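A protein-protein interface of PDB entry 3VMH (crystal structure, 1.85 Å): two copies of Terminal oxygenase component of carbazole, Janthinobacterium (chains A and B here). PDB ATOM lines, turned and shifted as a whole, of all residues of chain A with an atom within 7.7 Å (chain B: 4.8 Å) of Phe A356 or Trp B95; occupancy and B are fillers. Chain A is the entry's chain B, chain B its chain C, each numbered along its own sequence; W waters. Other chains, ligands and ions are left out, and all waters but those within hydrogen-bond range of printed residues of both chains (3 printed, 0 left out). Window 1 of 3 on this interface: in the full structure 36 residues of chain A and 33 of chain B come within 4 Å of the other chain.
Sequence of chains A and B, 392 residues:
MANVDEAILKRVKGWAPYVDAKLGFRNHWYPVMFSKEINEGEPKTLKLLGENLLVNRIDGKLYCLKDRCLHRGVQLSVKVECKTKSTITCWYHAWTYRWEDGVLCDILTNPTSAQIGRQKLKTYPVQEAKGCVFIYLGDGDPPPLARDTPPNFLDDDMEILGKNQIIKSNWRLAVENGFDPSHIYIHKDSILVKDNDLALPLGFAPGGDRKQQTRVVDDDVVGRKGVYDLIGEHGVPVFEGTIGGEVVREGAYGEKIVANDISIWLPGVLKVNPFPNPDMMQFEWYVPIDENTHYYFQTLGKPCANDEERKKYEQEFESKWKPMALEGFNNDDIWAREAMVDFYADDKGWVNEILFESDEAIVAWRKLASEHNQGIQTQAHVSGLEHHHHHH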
ATOM      1  N   ASP A 180     -36.787  15.416   4.233  1.00  0.00           N
ATOM      2  CA  ASP A 180     -35.634  14.741   3.625  1.00  0.00           C
ATOM      3  C   ASP A 180     -34.322  15.265   4.234  1.00  0.00           C
ATOM      4  O   ASP A 180     -33.915  16.393   3.959  1.00  0.00           O
ATOM      5  CB  ASP A 180     -35.655  15.024   2.117  1.00  0.00           C
ATOM      6  CG  ASP A 180     -34.659  14.194   1.336  1.00  0.00           C
ATOM      7  OD1 ASP A 180     -33.547  13.937   1.838  1.00  0.00           O
ATOM      8  OD2 ASP A 180     -34.989  13.814   0.194  1.00  0.00           O
ATOM      9  N   PRO A 181     -33.635  14.447   5.047  1.00  0.00           N
ATOM     10  CA  PRO A 181     -32.380  14.898   5.663  1.00  0.00           C
ATOM     11  C   PRO A 181     -31.286  15.336   4.686  1.00  0.00           C
ATOM     12  O   PRO A 181     -30.612  16.343   4.911  1.00  0.00           O
ATOM     13  CB  PRO A 181     -31.945  13.685   6.496  1.00  0.00           C
ATOM     14  CG  PRO A 181     -33.244  12.993   6.808  1.00  0.00           C
ATOM     15  CD  PRO A 181     -33.967  13.080   5.484  1.00  0.00           C
ATOM     16  N   SER A 182     -31.120  14.589   3.603  1.00  0.00           N
ATOM     17  CA  SER A 182     -30.075  14.899   2.628  1.00  0.00           C
ATOM     18  C   SER A 182     -30.379  15.976   1.590  1.00  0.00           C
ATOM     19  O   SER A 182     -29.475  16.390   0.867  1.00  0.00           O
ATOM     20  CB  SER A 182     -29.648  13.626   1.901  1.00  0.00           C
ATOM     21  OG  SER A 182     -29.011  12.730   2.788  1.00  0.00           O
ATOM     22  N   HIS A 183     -31.626  16.437   1.509  1.00  0.00           N
ATOM     23  CA  HIS A 183     -31.967  17.456   0.519  1.00  0.00           C
ATOM     24  C   HIS A 183     -31.359  18.808   0.872  1.00  0.00           C
ATOM     25  O   HIS A 183     -31.444  19.760   0.097  1.00  0.00           O
ATOM     26  CB  HIS A 183     -33.490  17.587   0.357  1.00  0.00           C
ATOM     27  CG  HIS A 183     -34.104  18.675   1.180  1.00  0.00           C
ATOM     28  ND1 HIS A 183     -34.356  18.541   2.528  1.00  0.00           N
ATOM     29  CD2 HIS A 183     -34.517  19.920   0.843  1.00  0.00           C
ATOM     30  CE1 HIS A 183     -34.900  19.655   2.986  1.00  0.00           C
ATOM     31  NE2 HIS A 183     -35.007  20.508   1.983  1.00  0.00           N
ATOM     32  N   TYR A 185     -28.627  19.618   0.656  1.00  0.00           N
ATOM     33  CA  TYR A 185     -27.653  19.885  -0.395  1.00  0.00           C
ATOM     34  C   TYR A 185     -28.124  20.962  -1.379  1.00  0.00           C
ATOM     35  O   TYR A 185     -27.308  21.724  -1.903  1.00  0.00           O
ATOM     36  CB  TYR A 185     -27.361  18.587  -1.154  1.00  0.00           C
ATOM     37  CG  TYR A 185     -26.297  18.716  -2.221  1.00  0.00           C
ATOM     38  CD1 TYR A 185     -24.949  18.800  -1.880  1.00  0.00           C
ATOM     39  CD2 TYR A 185     -26.642  18.784  -3.572  1.00  0.00           C
ATOM     40  CE1 TYR A 185     -23.964  18.948  -2.858  1.00  0.00           C
ATOM     41  CE2 TYR A 185     -25.668  18.934  -4.556  1.00  0.00           C
ATOM     42  CZ  TYR A 185     -24.330  19.016  -4.192  1.00  0.00           C
ATOM     43  OH  TYR A 185     -23.360  19.175  -5.159  1.00  0.00           O
ATOM     44  N   PHE A 204     -25.152  14.003   5.537  1.00  0.00           N
ATOM     45  CA  PHE A 204     -24.817  13.277   6.755  1.00  0.00           C
ATOM     46  C   PHE A 204     -24.401  11.837   6.501  1.00  0.00           C
ATOM     47  O   PHE A 204     -24.975  11.153   5.655  1.00  0.00           O
ATOM     48  CB  PHE A 204     -26.022  13.246   7.695  1.00  0.00           C
ATOM     49  CG  PHE A 204     -26.574  14.596   8.025  1.00  0.00           C
ATOM     50  CD1 PHE A 204     -26.089  15.314   9.113  1.00  0.00           C
ATOM     51  CD2 PHE A 204     -27.586  15.152   7.249  1.00  0.00           C
ATOM     52  CE1 PHE A 204     -26.605  16.569   9.426  1.00  0.00           C
ATOM     53  CE2 PHE A 204     -28.108  16.401   7.548  1.00  0.00           C
ATOM     54  CZ  PHE A 204     -27.618  17.115   8.642  1.00  0.00           C
ATOM     55  N   PRO A 206     -24.705   8.666   8.246  1.00  0.00           N
ATOM     56  CA  PRO A 206     -25.447   8.101   9.379  1.00  0.00           C
ATOM     57  C   PRO A 206     -24.681   7.139  10.276  1.00  0.00           C
ATOM     58  O   PRO A 206     -23.724   6.490   9.851  1.00  0.00           O
ATOM     59  CB  PRO A 206     -26.644   7.438   8.705  1.00  0.00           C
ATOM     60  CG  PRO A 206     -26.063   6.974   7.402  1.00  0.00           C
ATOM     61  CD  PRO A 206     -25.236   8.164   6.966  1.00  0.00           C
ATOM     62  N   GLU A 353     -38.441   4.041  -7.293  1.00  0.00           N
ATOM     63  CA  GLU A 353     -37.490   4.879  -6.560  1.00  0.00           C
ATOM     64  C   GLU A 353     -36.388   4.003  -5.944  1.00  0.00           C
ATOM     65  O   GLU A 353     -36.663   2.911  -5.450  1.00  0.00           O
ATOM     66  CB  GLU A 353     -38.222   5.610  -5.430  1.00  0.00           C
ATOM     67  CG  GLU A 353     -38.885   4.634  -4.460  1.00  0.00           C
ATOM     68  CD  GLU A 353     -39.743   5.301  -3.398  1.00  0.00           C
ATOM     69  OE1 GLU A 353     -39.976   6.521  -3.477  1.00  0.00           O
ATOM     70  OE2 GLU A 353     -40.193   4.585  -2.482  1.00  0.00           O
ATOM     71  N   ILE A 354     -35.144   4.471  -5.987  1.00  0.00           N
ATOM     72  CA  ILE A 354     -34.038   3.725  -5.386  1.00  0.00           C
ATOM     73  C   ILE A 354     -33.553   4.580  -4.217  1.00  0.00           C
ATOM     74  O   ILE A 354     -32.838   5.562  -4.398  1.00  0.00           O
ATOM     75  CB  ILE A 354     -32.895   3.477  -6.401  1.00  0.00           C
ATOM     76  CG1 ILE A 354     -33.388   2.529  -7.503  1.00  0.00           C
ATOM     77  CG2 ILE A 354     -31.683   2.869  -5.691  1.00  0.00           C
ATOM     78  CD1 ILE A 354     -32.374   2.266  -8.609  1.00  0.00           C
ATOM     79  N   LEU A 355     -33.969   4.194  -3.015  1.00  0.00           N
ATOM     80  CA  LEU A 355     -33.641   4.931  -1.802  1.00  0.00           C
ATOM     81  C   LEU A 355     -32.276   4.597  -1.220  1.00  0.00           C
ATOM     82  O   LEU A 355     -31.722   3.535  -1.493  1.00  0.00           O
ATOM     83  CB  LEU A 355     -34.705   4.647  -0.731  1.00  0.00           C
ATOM     84  CG  LEU A 355     -36.173   4.724  -1.170  1.00  0.00           C
ATOM     85  CD1 LEU A 355     -37.097   4.312  -0.028  1.00  0.00           C
ATOM     86  CD2 LEU A 355     -36.482   6.136  -1.619  1.00  0.00           C
ATOM     87  N   PHE A 356     -31.735   5.521  -0.428  1.00  0.00           N
ATOM     88  CA  PHE A 356     -30.472   5.271   0.251  1.00  0.00           C
ATOM     89  C   PHE A 356     -30.663   5.572   1.738  1.00  0.00           C
ATOM     90  O   PHE A 356     -31.760   5.948   2.155  1.00  0.00           O
ATOM     91  CB  PHE A 356     -29.294   6.039  -0.398  1.00  0.00           C
ATOM     92  CG  PHE A 356     -29.251   7.520  -0.129  1.00  0.00           C
ATOM     93  CD1 PHE A 356     -30.401   8.295  -0.106  1.00  0.00           C
ATOM     94  CD2 PHE A 356     -28.016   8.158  -0.019  1.00  0.00           C
ATOM     95  CE1 PHE A 356     -30.328   9.683   0.012  1.00  0.00           C
ATOM     96  CE2 PHE A 356     -27.931   9.552   0.100  1.00  0.00           C
ATOM     97  CZ  PHE A 356     -29.091  10.313   0.112  1.00  0.00           C
ATOM     98  N   GLU A 357     -29.617   5.380   2.535  1.00  0.00           N
ATOM     99  CA  GLU A 357     -29.701   5.547   3.990  1.00  0.00           C
ATOM    100  C   GLU A 357     -30.563   6.633   4.640  1.00  0.00           C
ATOM    101  O   GLU A 357     -31.449   6.315   5.442  1.00  0.00           O
ATOM    102  CB  GLU A 357     -28.292   5.614   4.588  1.00  0.00           C
ATOM    103  CG  GLU A 357     -27.513   4.307   4.494  1.00  0.00           C
ATOM    104  CD  GLU A 357     -26.948   4.036   3.105  1.00  0.00           C
ATOM    105  OE1 GLU A 357     -27.029   4.926   2.234  1.00  0.00           O
ATOM    106  OE2 GLU A 357     -26.413   2.929   2.889  1.00  0.00           O
ATOM    107  N   SER A 358     -30.320   7.899   4.329  1.00  0.00           N
ATOM    108  CA  SER A 358     -31.086   8.969   4.953  1.00  0.00           C
ATOM    109  C   SER A 358     -32.591   8.926   4.681  1.00  0.00           C
ATOM    110  O   SER A 358     -33.367   9.578   5.379  1.00  0.00           O
ATOM    111  CB  SER A 358     -30.522  10.340   4.554  1.00  0.00           C
ATOM    112  OG  SER A 358     -30.583  10.548   3.154  1.00  0.00           O
ATOM    113  N   ASP A 359     -33.009   8.147   3.686  1.00  0.00           N
ATOM    114  CA  ASP A 359     -34.428   8.050   3.374  1.00  0.00           C
ATOM    115  C   ASP A 359     -35.187   7.265   4.438  1.00  0.00           C
ATOM    116  O   ASP A 359     -36.409   7.123   4.370  1.00  0.00           O
ATOM    117  CB  ASP A 359     -34.628   7.425   1.993  1.00  0.00           C
ATOM    118  CG  ASP A 359     -34.180   8.350   0.876  1.00  0.00           C
ATOM    119  OD1 ASP A 359     -34.408   9.572   1.007  1.00  0.00           O
ATOM    120  OD2 ASP A 359     -33.613   7.866  -0.122  1.00  0.00           O
ATOM    121  N   GLU A 360     -34.452   6.759   5.422  1.00  0.00           N
ATOM    122  CA  GLU A 360     -35.055   6.016   6.516  1.00  0.00           C
ATOM    123  C   GLU A 360     -36.083   6.938   7.167  1.00  0.00           C
ATOM    124  O   GLU A 360     -37.130   6.492   7.630  1.00  0.00           O
ATOM    125  CB  GLU A 360     -33.978   5.626   7.532  1.00  0.00           C
ATOM    126  CG  GLU A 360     -34.388   4.518   8.473  1.00  0.00           C
ATOM    127  CD  GLU A 360     -34.627   3.205   7.746  1.00  0.00           C
ATOM    128  OE1 GLU A 360     -33.659   2.632   7.189  1.00  0.00           O
ATOM    129  OE2 GLU A 360     -35.786   2.750   7.731  1.00  0.00           O
ATOM    130  N   ALA A 361     -35.776   8.231   7.194  1.00  0.00           N
ATOM    131  CA  ALA A 361     -36.679   9.218   7.772  1.00  0.00           C
ATOM    132  C   ALA A 361     -37.983   9.266   6.976  1.00  0.00           C
ATOM    133  O   ALA A 361     -39.072   9.275   7.549  1.00  0.00           O
ATOM    134  CB  ALA A 361     -36.021  10.597   7.780  1.00  0.00           C
ATOM    135  N   ILE A 362     -37.868   9.295   5.653  1.00  0.00           N
ATOM    136  CA  ILE A 362     -39.053   9.349   4.805  1.00  0.00           C
ATOM    137  C   ILE A 362     -39.896   8.085   4.976  1.00  0.00           C
ATOM    138  O   ILE A 362     -41.121   8.160   5.060  1.00  0.00           O
ATOM    139  CB  ILE A 362     -38.659   9.546   3.324  1.00  0.00           C
ATOM    140  CG1 ILE A 362     -38.065  10.953   3.146  1.00  0.00           C
ATOM    141  CG2 ILE A 362     -39.871   9.343   2.415  1.00  0.00           C
ATOM    142  CD1 ILE A 362     -37.591  11.268   1.739  1.00  0.00           C
ATOM    143  N   VAL A 363     -39.237   6.932   5.045  1.00  0.00           N
ATOM    144  CA  VAL A 363     -39.942   5.667   5.224  1.00  0.00           C
ATOM    145  C   VAL A 363     -40.717   5.669   6.539  1.00  0.00           C
ATOM    146  O   VAL A 363     -41.854   5.194   6.598  1.00  0.00           O
ATOM    147  CB  VAL A 363     -38.961   4.467   5.218  1.00  0.00           C
ATOM    148  CG1 VAL A 363     -39.667   3.209   5.711  1.00  0.00           C
ATOM    149  CG2 VAL A 363     -38.427   4.245   3.803  1.00  0.00           C
ATOM    150  N   CYS B  69     -32.280  10.784 -12.522  1.00  0.00           N
ATOM    151  CA  CYS B  69     -31.548  10.257 -11.378  1.00  0.00           C
ATOM    152  C   CYS B  69     -32.188   8.968 -10.873  1.00  0.00           C
ATOM    153  O   CYS B  69     -33.411   8.854 -10.818  1.00  0.00           O
ATOM    154  CB  CYS B  69     -31.525  11.292 -10.259  1.00  0.00           C
ATOM    155  SG  CYS B  69     -30.436  10.862  -8.879  1.00  0.00           S
ATOM    156  N   LEU B  70     -31.351   8.006 -10.499  1.00  0.00           N
ATOM    157  CA  LEU B  70     -31.817   6.721  -9.988  1.00  0.00           C
ATOM    158  C   LEU B  70     -32.560   6.855  -8.661  1.00  0.00           C
ATOM    159  O   LEU B  70     -33.425   6.039  -8.337  1.00  0.00           O
ATOM    160  CB  LEU B  70     -30.627   5.771  -9.771  1.00  0.00           C
ATOM    161  CG  LEU B  70     -29.797   5.329 -10.980  1.00  0.00           C
ATOM    162  CD1 LEU B  70     -28.667   4.416 -10.507  1.00  0.00           C
ATOM    163  CD2 LEU B  70     -30.678   4.591 -11.976  1.00  0.00           C
ATOM    164  N   HIS B  71     -32.209   7.884  -7.901  1.00  0.00           N
ATOM    165  CA  HIS B  71     -32.784   8.114  -6.581  1.00  0.00           C
ATOM    166  C   HIS B  71     -34.273   8.459  -6.565  1.00  0.00           C
ATOM    167  O   HIS B  71     -35.109   7.586  -6.323  1.00  0.00           O
ATOM    168  CB  HIS B  71     -31.984   9.207  -5.867  1.00  0.00           C
ATOM    169  CG  HIS B  71     -32.341   9.377  -4.424  1.00  0.00           C
ATOM    170  ND1 HIS B  71     -32.227  10.582  -3.769  1.00  0.00           N
ATOM    171  CD2 HIS B  71     -32.806   8.493  -3.508  1.00  0.00           C
ATOM    172  CE1 HIS B  71     -32.610  10.437  -2.512  1.00  0.00           C
ATOM    173  NE2 HIS B  71     -32.966   9.178  -2.329  1.00  0.00           N
ATOM    174  N   ILE B  88     -21.071  13.752 -13.409  1.00  0.00           N
ATOM    175  CA  ILE B  88     -22.164  14.699 -13.274  1.00  0.00           C
ATOM    176  C   ILE B  88     -22.799  14.389 -11.924  1.00  0.00           C
ATOM    177  O   ILE B  88     -23.000  13.224 -11.576  1.00  0.00           O
ATOM    178  CB  ILE B  88     -23.224  14.565 -14.405  1.00  0.00           C
ATOM    179  CG1 ILE B  88     -24.350  15.573 -14.164  1.00  0.00           C
ATOM    180  CG2 ILE B  88     -23.765  13.149 -14.465  1.00  0.00           C
ATOM    181  CD1 ILE B  88     -25.331  15.728 -15.321  1.00  0.00           C
ATOM    182  N   THR B  89     -23.096  15.436 -11.167  1.00  0.00           N
ATOM    183  CA  THR B  89     -23.680  15.290  -9.835  1.00  0.00           C
ATOM    184  C   THR B  89     -25.119  15.781  -9.788  1.00  0.00           C
ATOM    185  O   THR B  89     -25.393  16.938 -10.104  1.00  0.00           O
ATOM    186  CB  THR B  89     -22.848  16.084  -8.796  1.00  0.00           C
ATOM    187  OG1 THR B  89     -21.543  15.505  -8.695  1.00  0.00           O
ATOM    188  CG2 THR B  89     -23.520  16.067  -7.426  1.00  0.00           C
ATOM    189  N   CYS B  90     -26.040  14.911  -9.382  1.00  0.00           N
ATOM    190  CA  CYS B  90     -27.440  15.313  -9.291  1.00  0.00           C
ATOM    191  C   CYS B  90     -27.545  16.474  -8.316  1.00  0.00           C
ATOM    192  O   CYS B  90     -26.940  16.456  -7.243  1.00  0.00           O
ATOM    193  CB  CYS B  90     -28.322  14.156  -8.806  1.00  0.00           C
ATOM    194  SG  CYS B  90     -30.082  14.592  -8.731  1.00  0.00           S
ATOM    195  N   HIS B  93     -29.562  15.296  -4.214  1.00  0.00           N
ATOM    196  CA  HIS B  93     -28.854  14.708  -3.077  1.00  0.00           C
ATOM    197  C   HIS B  93     -27.426  14.331  -3.452  1.00  0.00           C
ATOM    198  O   HIS B  93     -26.780  13.529  -2.781  1.00  0.00           O
ATOM    199  CB  HIS B  93     -29.605  13.481  -2.551  1.00  0.00           C
ATOM    200  CG  HIS B  93     -31.068  13.715  -2.346  1.00  0.00           C
ATOM    201  ND1 HIS B  93     -31.993  13.563  -3.358  1.00  0.00           N
ATOM    202  CD2 HIS B  93     -31.766  14.105  -1.253  1.00  0.00           C
ATOM    203  CE1 HIS B  93     -33.197  13.846  -2.894  1.00  0.00           C
ATOM    204  NE2 HIS B  93     -33.088  14.178  -1.620  1.00  0.00           N
ATOM    205  N   ALA B  94     -26.959  14.897  -4.558  1.00  0.00           N
ATOM    206  CA  ALA B  94     -25.591  14.700  -5.025  1.00  0.00           C
ATOM    207  C   ALA B  94     -25.100  13.307  -5.414  1.00  0.00           C
ATOM    208  O   ALA B  94     -23.903  13.018  -5.286  1.00  0.00           O
ATOM    209  CB  ALA B  94     -24.627  15.321  -4.008  1.00  0.00           C
ATOM    210  N   TRP B  95     -25.995  12.435  -5.877  1.00  0.00           N
ATOM    211  CA  TRP B  95     -25.563  11.121  -6.333  1.00  0.00           C
ATOM    212  C   TRP B  95     -24.739  11.461  -7.575  1.00  0.00           C
ATOM    213  O   TRP B  95     -25.201  12.200  -8.446  1.00  0.00           O
ATOM    214  CB  TRP B  95     -26.766  10.256  -6.719  1.00  0.00           C
ATOM    215  CG  TRP B  95     -27.466   9.644  -5.541  1.00  0.00           C
ATOM    216  CD1 TRP B  95     -27.594  10.182  -4.293  1.00  0.00           C
ATOM    217  CD2 TRP B  95     -28.174   8.402  -5.519  1.00  0.00           C
ATOM    218  NE1 TRP B  95     -28.345   9.350  -3.491  1.00  0.00           N
ATOM    219  CE2 TRP B  95     -28.713   8.251  -4.219  1.00  0.00           C
ATOM    220  CE3 TRP B  95     -28.408   7.399  -6.470  1.00  0.00           C
ATOM    221  CZ2 TRP B  95     -29.475   7.136  -3.847  1.00  0.00           C
ATOM    222  CZ3 TRP B  95     -29.167   6.286  -6.098  1.00  0.00           C
ATOM    223  CH2 TRP B  95     -29.690   6.168  -4.795  1.00  0.00           C
ATOM    224  N   THR B  96     -23.528  10.925  -7.652  1.00  0.00           N
ATOM    225  CA  THR B  96     -22.627  11.231  -8.758  1.00  0.00           C
ATOM    226  C   THR B  96     -22.350  10.053  -9.679  1.00  0.00           C
ATOM    227  O   THR B  96     -21.985   8.967  -9.234  1.00  0.00           O
ATOM    228  CB  THR B  96     -21.313  11.801  -8.190  1.00  0.00           C
ATOM    229  OG1 THR B  96     -21.619  12.969  -7.416  1.00  0.00           O
ATOM    230  CG2 THR B  96     -20.340  12.174  -9.308  1.00  0.00           C
ATOM    231  N   TYR B  97     -22.521  10.281 -10.978  1.00  0.00           N
ATOM    232  CA  TYR B  97     -22.318   9.238 -11.971  1.00  0.00           C
ATOM    233  C   TYR B  97     -21.208   9.575 -12.958  1.00  0.00           C
ATOM    234  O   TYR B  97     -20.968  10.739 -13.266  1.00  0.00           O
ATOM    235  CB  TYR B  97     -23.602   9.003 -12.773  1.00  0.00           C
ATOM    236  CG  TYR B  97     -24.870   8.915 -11.953  1.00  0.00           C
ATOM    237  CD1 TYR B  97     -25.550  10.065 -11.558  1.00  0.00           C
ATOM    238  CD2 TYR B  97     -25.397   7.680 -11.586  1.00  0.00           C
ATOM    239  CE1 TYR B  97     -26.729   9.989 -10.819  1.00  0.00           C
ATOM    240  CE2 TYR B  97     -26.573   7.589 -10.850  1.00  0.00           C
ATOM    241  CZ  TYR B  97     -27.233   8.746 -10.472  1.00  0.00           C
ATOM    242  OH  TYR B  97     -28.405   8.649  -9.759  1.00  0.00           O
ATOM    243  N   LEU B 104     -22.652   4.797 -10.410  1.00  0.00           N
ATOM    244  CA  LEU B 104     -22.815   5.717  -9.293  1.00  0.00           C
ATOM    245  C   LEU B 104     -21.485   5.567  -8.548  1.00  0.00           C
ATOM    246  O   LEU B 104     -21.289   4.603  -7.805  1.00  0.00           O
ATOM    247  CB  LEU B 104     -23.980   5.261  -8.406  1.00  0.00           C
ATOM    248  CG  LEU B 104     -24.232   6.021  -7.102  1.00  0.00           C
ATOM    249  CD1 LEU B 104     -24.510   7.491  -7.386  1.00  0.00           C
ATOM    250  CD2 LEU B 104     -25.404   5.379  -6.375  1.00  0.00           C
ATOM    251  N   ASP B 106     -19.954   8.111  -6.528  1.00  0.00           N
ATOM    252  CA  ASP B 106     -19.872   8.892  -5.295  1.00  0.00           C
ATOM    253  C   ASP B 106     -21.233   9.485  -4.929  1.00  0.00           C
ATOM    254  O   ASP B 106     -22.123   9.593  -5.769  1.00  0.00           O
ATOM    255  CB  ASP B 106     -18.881  10.055  -5.452  1.00  0.00           C
ATOM    256  CG  ASP B 106     -17.429   9.618  -5.369  1.00  0.00           C
ATOM    257  OD1 ASP B 106     -16.984   9.207  -4.275  1.00  0.00           O
ATOM    258  OD2 ASP B 106     -16.730   9.695  -6.401  1.00  0.00           O
ATOM    259  N   ILE B 107     -21.377   9.864  -3.664  1.00  0.00           N
ATOM    260  CA  ILE B 107     -22.594  10.500  -3.171  1.00  0.00           C
ATOM    261  C   ILE B 107     -22.121  11.500  -2.128  1.00  0.00           C
ATOM    262  O   ILE B 107     -21.787  11.128  -1.002  1.00  0.00           O
ATOM    263  CB  ILE B 107     -23.569   9.494  -2.519  1.00  0.00           C
ATOM    264  CG1 ILE B 107     -23.981   8.423  -3.538  1.00  0.00           C
ATOM    265  CG2 ILE B 107     -24.801  10.240  -2.010  1.00  0.00           C
ATOM    266  CD1 ILE B 107     -25.002   7.415  -3.014  1.00  0.00           C
ATOM    267  N   THR B 109     -23.659  13.668  -0.320  1.00  0.00           N
ATOM    268  CA  THR B 109     -24.465  13.797   0.889  1.00  0.00           C
ATOM    269  C   THR B 109     -24.258  12.643   1.869  1.00  0.00           C
ATOM    270  O   THR B 109     -24.698  12.716   3.019  1.00  0.00           O
ATOM    271  CB  THR B 109     -25.973  13.891   0.558  1.00  0.00           C
ATOM    272  OG1 THR B 109     -26.376  12.734  -0.184  1.00  0.00           O
ATOM    273  CG2 THR B 109     -26.264  15.150  -0.247  1.00  0.00           C
ATOM    274  N   ASN B 110     -23.602  11.579   1.417  1.00  0.00           N
ATOM    275  CA  ASN B 110     -23.341  10.420   2.273  1.00  0.00           C
ATOM    276  C   ASN B 110     -22.246   9.547   1.674  1.00  0.00           C
ATOM    277  O   ASN B 110     -22.523   8.554   1.003  1.00  0.00           O
ATOM    278  CB  ASN B 110     -24.610   9.582   2.463  1.00  0.00           C
ATOM    279  CG  ASN B 110     -24.406   8.426   3.436  1.00  0.00           C
ATOM    280  OD1 ASN B 110     -25.298   7.599   3.628  1.00  0.00           O
ATOM    281  ND2 ASN B 110     -23.229   8.368   4.057  1.00  0.00           N
ATOM    282  N   SER B 113     -22.525   5.711   2.078  1.00  0.00           N
ATOM    283  CA  SER B 113     -23.666   4.981   1.542  1.00  0.00           C
ATOM    284  C   SER B 113     -23.308   3.662   0.866  1.00  0.00           C
ATOM    285  O   SER B 113     -22.333   3.571   0.117  1.00  0.00           O
ATOM    286  CB  SER B 113     -24.442   5.852   0.552  1.00  0.00           C
ATOM    287  OG  SER B 113     -25.537   5.121   0.031  1.00  0.00           O
ATOM    288  N   GLN B 115     -24.947   2.326  -1.415  1.00  0.00           N
ATOM    289  CA  GLN B 115     -25.342   2.386  -2.821  1.00  0.00           C
ATOM    290  C   GLN B 115     -24.156   2.712  -3.720  1.00  0.00           C
ATOM    291  O   GLN B 115     -24.162   2.393  -4.905  1.00  0.00           O
ATOM    292  CB  GLN B 115     -26.431   3.445  -3.036  1.00  0.00           C
ATOM    293  CG  GLN B 115     -27.756   3.136  -2.354  1.00  0.00           C
ATOM    294  CD  GLN B 115     -28.450   1.924  -2.942  1.00  0.00           C
ATOM    295  OE1 GLN B 115     -27.814   1.049  -3.529  1.00  0.00           O
ATOM    296  NE2 GLN B 115     -29.769   1.858  -2.771  1.00  0.00           N
HETATM  297  O   HOH W   1     -27.982   8.557   3.085  1.00  0.00           O
HETATM  298  O   HOH W   2     -35.137  11.419  -0.870  1.00  0.00           O
HETATM  299  O   HOH W   3     -27.276  11.100   4.352  1.00  0.00           O
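Among the printed residues, pairs that only touch across the chains: Ser A182 with His B93 (3.7 Å), Ser A182 with Thr B109 (3.6 Å), His A183 with His B93 (3.6 Å), Tyr A185 with Thr B89 (3.9 Å), Tyr A185 with Cys B90 (3.9 Å), Tyr A185 with Ala B94 (3.7 Å), Tyr A185 with Thr B109 (3.7 Å), Phe A204 with Asn B110 (3.6 Å), Pro A206 with Asn B110 (3.4 Å), Glu A353 with His B71 (3.6 Å), Ile A354 with Trp B95 (3.2 Å), Ile A354 with Gln B115 (3.6 Å), Phe A356 with His B71 (3.5 Å), Phe A356 with Trp B95 (3.6 Å), Phe A356 with Ile B107 (3.8 Å), Phe A356 with Thr B109 (3.6 Å), Phe A356 with Ser B113 (3.9 Å) and Phe A356 with Gln B115 (3.8 Å).
OD1 of Asp A180 sits at hydrogen-bond distance from N of Ser A182 (3.1 Å).
The side-chain hydroxyl of Ser B113 sits close to the backbone NH of Gln B115 (3.2 Å).
The side-chain carboxylate (OE1) of Glu A357 sits close to the side-chain amide oxygen (OD1) of Asn B110.
The backbone NH of Ile A354 lies close to the backbone carbonyl oxygen of Leu B70, 3.3 Å away.
The backbone NH (N) of Phe A204 is in hydrogen-bond range of the backbone carbonyl oxygen (O) of Thr B109, 2.9 Å away.
OD2 of Asp A359 is in hydrogen-bond range of NE2 of His B71.
The backbone carbonyl oxygen (O) of Leu A355 is in hydrogen-bond range of the side-chain amide nitrogen (NE2) of Gln B115.
N of Ile A354 is in hydrogen-bond range of O of His B71 (3.1 Å).
OE1 of Glu A357 is in hydrogen-bond range of OG of Ser B113 (2.7 Å).
OD2 of Asp A180 sits at hydrogen-bond distance from NE2 of His B93 (2.7 Å).
Water W2 lies within hydrogen-bond range of the side-chain carboxylate of Asp A180 (2.6 Å), the side-chain carboxylate of Asp A359 (2.7 Å) and a ring nitrogen (NE2) of His B71 (3.4 Å).
Water W1 bridges N of Ser A358 and OD1 of Asn B110.
Phe A356 touches just these residues of chain B: His B71 (3.5 Å), Trp B95 (3.6 Å), Ile B107 (3.8 Å), Thr B109 (3.6 Å), Ser B113 (3.9 Å) and Gln B115 (3.8 Å).
Of the printed residues of chain A, His B93 touches Asp A180, Ser A182 and His A183.
Printed residues of chain A within 4 Å of Ala B94: Tyr A185 (3.7 Å).
Of chain A, only Ile A354 and Phe A356 come within 4 Å of Trp B95.
Of the printed residues of chain A, Gln B115 touches Ile A354, Leu A355 and Phe A356.
The nearest residue of chain B that does not touch Phe A356 is Asn B110 (4.1 Å).
The nearest residue of chain A that does not touch Trp B95 is Leu A355 (4.6 Å).
Of the 18 printed residues of chain A, 12 touch a printed residue of chain B.
Hydrophobic or aromatic side chains of chain B within 4 Å of the printed part of chain A: His B71, His B93, Ala B94, Trp B95 and Ile B107.
Among the printed residues, 26 pairs touch across the chains.
Among the printed residues, no Asp or Glu carboxylate lies within 4 Å of a Lys or Arg side-chain nitrogen of the other chain.
No position is printed for both chains.
Of the 26 pairs that touch across the chains among the printed residues, none has its exchanged pair printed and touching as well.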
